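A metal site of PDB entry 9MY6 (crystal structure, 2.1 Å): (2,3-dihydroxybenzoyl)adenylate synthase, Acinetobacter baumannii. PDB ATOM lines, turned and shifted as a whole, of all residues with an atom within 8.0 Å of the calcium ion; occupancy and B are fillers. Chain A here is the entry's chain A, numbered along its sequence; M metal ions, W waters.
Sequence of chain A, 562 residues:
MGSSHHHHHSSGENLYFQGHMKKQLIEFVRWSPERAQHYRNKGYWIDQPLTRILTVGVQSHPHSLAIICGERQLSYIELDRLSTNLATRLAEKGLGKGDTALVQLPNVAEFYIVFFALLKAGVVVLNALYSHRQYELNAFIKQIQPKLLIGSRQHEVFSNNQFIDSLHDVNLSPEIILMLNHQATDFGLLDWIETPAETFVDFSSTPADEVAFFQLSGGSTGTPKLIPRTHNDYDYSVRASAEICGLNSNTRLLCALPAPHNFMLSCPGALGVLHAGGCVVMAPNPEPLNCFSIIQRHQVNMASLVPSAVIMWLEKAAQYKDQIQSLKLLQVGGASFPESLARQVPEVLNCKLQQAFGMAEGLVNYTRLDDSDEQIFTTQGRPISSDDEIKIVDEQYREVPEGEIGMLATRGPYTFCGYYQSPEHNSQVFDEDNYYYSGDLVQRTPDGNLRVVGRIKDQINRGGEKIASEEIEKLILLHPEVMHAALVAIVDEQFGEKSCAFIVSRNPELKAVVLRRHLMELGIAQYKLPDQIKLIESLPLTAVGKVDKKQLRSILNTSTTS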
ATOM      1  N   VAL A 300      -1.075  16.693  17.661  1.00  0.00           N
ATOM      2  CA  VAL A 300      -1.450  15.880  16.516  1.00  0.00           C
ATOM      3  C   VAL A 300      -0.440  16.103  15.409  1.00  0.00           C
ATOM      4  O   VAL A 300      -0.077  17.255  15.105  1.00  0.00           O
ATOM      5  CB  VAL A 300      -2.880  16.225  16.065  1.00  0.00           C
ATOM      6  CG1 VAL A 300      -3.180  15.680  14.702  1.00  0.00           C
ATOM      7  CG2 VAL A 300      -3.888  15.737  17.076  1.00  0.00           C
ATOM      8  N   ASN A 301       0.038  15.016  14.799  1.00  0.00           N
ATOM      9  CA  ASN A 301       1.040  15.158  13.741  1.00  0.00           C
ATOM     10  C   ASN A 301       0.540  14.664  12.395  1.00  0.00           C
ATOM     11  O   ASN A 301       1.266  14.802  11.403  1.00  0.00           O
ATOM     12  CB  ASN A 301       2.370  14.463  14.121  1.00  0.00           C
ATOM     13  CG  ASN A 301       2.180  13.023  14.612  1.00  0.00           C
ATOM     14  OD1 ASN A 301       1.286  12.295  14.154  1.00  0.00           O
ATOM     15  ND2 ASN A 301       3.027  12.606  15.539  1.00  0.00           N
ATOM     16  N   LYS A 321      -0.824  29.611  13.122  1.00  0.00           N
ATOM     17  CA  LYS A 321       0.287  28.726  12.763  1.00  0.00           C
ATOM     18  C   LYS A 321       0.711  27.854  13.932  1.00  0.00           C
ATOM     19  O   LYS A 321       0.973  26.647  13.779  1.00  0.00           O
ATOM     20  CB  LYS A 321       1.477  29.544  12.255  1.00  0.00           C
ATOM     21  CG  LYS A 321       1.697  29.458  10.747  1.00  0.00           C
ATOM     22  CD  LYS A 321       2.976  30.164  10.296  1.00  0.00           C
ATOM     23  N   ILE A 324      -1.145  24.635  14.903  1.00  0.00           N
ATOM     24  CA  ILE A 324      -1.027  23.469  14.032  1.00  0.00           C
ATOM     25  C   ILE A 324       0.427  23.177  13.651  1.00  0.00           C
ATOM     26  O   ILE A 324       0.696  22.449  12.706  1.00  0.00           O
ATOM     27  CB  ILE A 324      -1.933  23.626  12.787  1.00  0.00           C
ATOM     28  CG1 ILE A 324      -1.533  24.842  11.949  1.00  0.00           C
ATOM     29  CG2 ILE A 324      -3.371  23.781  13.196  1.00  0.00           C
ATOM     30  CD1 ILE A 324      -2.416  25.063  10.740  1.00  0.00           C
ATOM     31  N   GLN A 325       1.387  23.710  14.401  1.00  0.00           N
ATOM     32  CA  GLN A 325       2.768  23.489  13.994  1.00  0.00           C
ATOM     33  C   GLN A 325       3.097  22.003  13.983  1.00  0.00           C
ATOM     34  O   GLN A 325       3.889  21.563  13.138  1.00  0.00           O
ATOM     35  CB  GLN A 325       3.737  24.279  14.885  1.00  0.00           C
ATOM     36  CG  GLN A 325       3.669  23.943  16.368  1.00  0.00           C
ATOM     37  CD  GLN A 325       4.714  22.900  16.813  1.00  0.00           C
ATOM     38  OE1 GLN A 325       5.867  22.913  16.376  1.00  0.00           O
ATOM     39  NE2 GLN A 325       4.303  22.014  17.715  1.00  0.00           N
ATOM     40  N   SER A 326       2.445  21.214  14.854  1.00  0.00           N
ATOM     41  CA  SER A 326       2.874  19.835  15.052  1.00  0.00           C
ATOM     42  C   SER A 326       2.445  18.927  13.916  1.00  0.00           C
ATOM     43  O   SER A 326       2.901  17.790  13.848  1.00  0.00           O
ATOM     44  CB  SER A 326       2.353  19.269  16.393  1.00  0.00           C
ATOM     45  OG  SER A 326       0.935  19.237  16.421  1.00  0.00           O
ATOM     46  N   LEU A 327       1.603  19.403  13.016  1.00  0.00           N
ATOM     47  CA  LEU A 327       1.199  18.609  11.872  1.00  0.00           C
ATOM     48  C   LEU A 327       2.407  18.258  11.008  1.00  0.00           C
ATOM     49  O   LEU A 327       3.164  19.144  10.605  1.00  0.00           O
ATOM     50  CB  LEU A 327       0.168  19.350  11.044  1.00  0.00           C
ATOM     51  CG  LEU A 327      -1.264  19.368  11.560  1.00  0.00           C
ATOM     52  CD1 LEU A 327      -2.021  20.372  10.741  1.00  0.00           C
ATOM     53  CD2 LEU A 327      -1.947  18.017  11.462  1.00  0.00           C
ATOM     54  N   LYS A 328       2.588  16.981  10.698  1.00  0.00           N
ATOM     55  CA  LYS A 328       3.681  16.625   9.810  1.00  0.00           C
ATOM     56  C   LYS A 328       3.231  16.134   8.459  1.00  0.00           C
ATOM     57  O   LYS A 328       3.959  16.296   7.475  1.00  0.00           O
ATOM     58  CB  LYS A 328       4.575  15.569  10.475  1.00  0.00           C
ATOM     59  CG  LYS A 328       5.232  16.109  11.718  1.00  0.00           C
ATOM     60  CD  LYS A 328       6.239  15.127  12.282  1.00  0.00           C
ATOM     61  CE  LYS A 328       6.849  15.635  13.575  1.00  0.00           C
ATOM     62  NZ  LYS A 328       6.575  14.608  14.645  1.00  0.00           N
ATOM     63  N   LEU A 329       2.031  15.578   8.370  1.00  0.00           N
ATOM     64  CA  LEU A 329       1.540  15.050   7.123  1.00  0.00           C
ATOM     65  C   LEU A 329       0.043  15.273   7.080  1.00  0.00           C
ATOM     66  O   LEU A 329      -0.652  15.002   8.073  1.00  0.00           O
ATOM     67  CB  LEU A 329       1.847  13.560   6.989  1.00  0.00           C
ATOM     68  CG  LEU A 329       1.322  12.828   5.764  1.00  0.00           C
ATOM     69  CD1 LEU A 329       2.104  13.302   4.540  1.00  0.00           C
ATOM     70  CD2 LEU A 329       1.455  11.292   5.965  1.00  0.00           C
ATOM     71  N   PRO A 346       1.968  22.800   2.164  1.00  0.00           N
ATOM     72  CA  PRO A 346       3.279  22.986   2.841  1.00  0.00           C
ATOM     73  C   PRO A 346       3.621  24.446   3.132  1.00  0.00           C
ATOM     74  O   PRO A 346       4.212  24.740   4.182  1.00  0.00           O
ATOM     75  CB  PRO A 346       4.283  22.353   1.874  1.00  0.00           C
ATOM     76  CG  PRO A 346       3.533  22.171   0.564  1.00  0.00           C
ATOM     77  CD  PRO A 346       2.089  22.091   0.877  1.00  0.00           C
ATOM     78  N   LEU A 349       0.190  25.491   5.763  1.00  0.00           N
ATOM     79  CA  LEU A 349      -0.060  24.593   6.880  1.00  0.00           C
ATOM     80  C   LEU A 349       1.222  24.001   7.460  1.00  0.00           C
ATOM     81  O   LEU A 349       1.180  23.435   8.551  1.00  0.00           O
ATOM     82  CB  LEU A 349      -1.011  23.470   6.438  1.00  0.00           C
ATOM     83  CG  LEU A 349      -2.423  23.875   5.974  1.00  0.00           C
ATOM     84  CD1 LEU A 349      -3.257  22.657   5.494  1.00  0.00           C
ATOM     85  CD2 LEU A 349      -3.168  24.610   7.083  1.00  0.00           C
ATOM     86  N   ASN A 350       2.353  24.116   6.757  1.00  0.00           N
ATOM     87  CA  ASN A 350       3.653  23.744   7.299  1.00  0.00           C
ATOM     88  C   ASN A 350       3.735  22.250   7.591  1.00  0.00           C
ATOM     89  O   ASN A 350       4.214  21.819   8.647  1.00  0.00           O
ATOM     90  CB  ASN A 350       3.971  24.559   8.541  1.00  0.00           C
ATOM     91  CG  ASN A 350       4.238  26.000   8.220  1.00  0.00           C
ATOM     92  OD1 ASN A 350       5.002  26.306   7.299  1.00  0.00           O
ATOM     93  ND2 ASN A 350       3.604  26.890   8.955  1.00  0.00           N
ATOM     94  N   CYS A 351       3.231  21.444   6.662  1.00  0.00           N
ATOM     95  CA  CYS A 351       3.334  20.006   6.773  1.00  0.00           C
ATOM     96  C   CYS A 351       3.404  19.439   5.374  1.00  0.00           C
ATOM     97  O   CYS A 351       3.164  20.146   4.384  1.00  0.00           O
ATOM     98  CB  CYS A 351       2.154  19.429   7.548  1.00  0.00           C
ATOM     99  SG  CYS A 351       0.615  19.803   6.707  1.00  0.00           S
ATOM    100  N   LYS A 352       3.738  18.158   5.271  1.00  0.00           N
ATOM    101  CA  LYS A 352       3.820  17.527   3.978  1.00  0.00           C
ATOM    102  C   LYS A 352       2.438  17.155   3.478  1.00  0.00           C
ATOM    103  O   LYS A 352       1.486  16.960   4.253  1.00  0.00           O
ATOM    104  CB  LYS A 352       4.694  16.270   4.035  1.00  0.00           C
ATOM    105  CG  LYS A 352       6.195  16.563   4.061  1.00  0.00           C
ATOM    106  CD  LYS A 352       6.866  15.737   5.173  1.00  0.00           C
ATOM    107  CE  LYS A 352       6.385  14.256   5.148  1.00  0.00           C
ATOM    108  NZ  LYS A 352       6.374  13.552   6.484  1.00  0.00           N
HETATM  109 CA    CA M   1       4.594  21.160  10.792  1.00  0.00          CA
HETATM  110  O   HOH W   1       6.341  20.140   9.868  1.00  0.00           O
HETATM  111  O   HOH W   2       2.413  22.431  10.595  1.00  0.00           O
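N of Leu 327 sits at hydrogen-bond distance from O of Val 300.
Three residues have an atom within 4 Å of the calcium ion: Gln 325, Leu 327 and Asn 350.
The calcium ion is bound by water W1 (2.2 Å), the backbone carbonyl oxygen (O) of Asn 350 (2.3 Å), the backbone carbonyl oxygen (O) of Leu 327 (2.5 Å), the backbone carbonyl oxygen (O) of Gln 325 (2.5 Å) and water W2 (2.5 Å).
Water W2 lies within hydrogen-bond range of the backbone carbonyl oxygen of Leu 349 (2.6 Å) and the backbone carbonyl oxygen of Ile 324 (2.7 Å).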
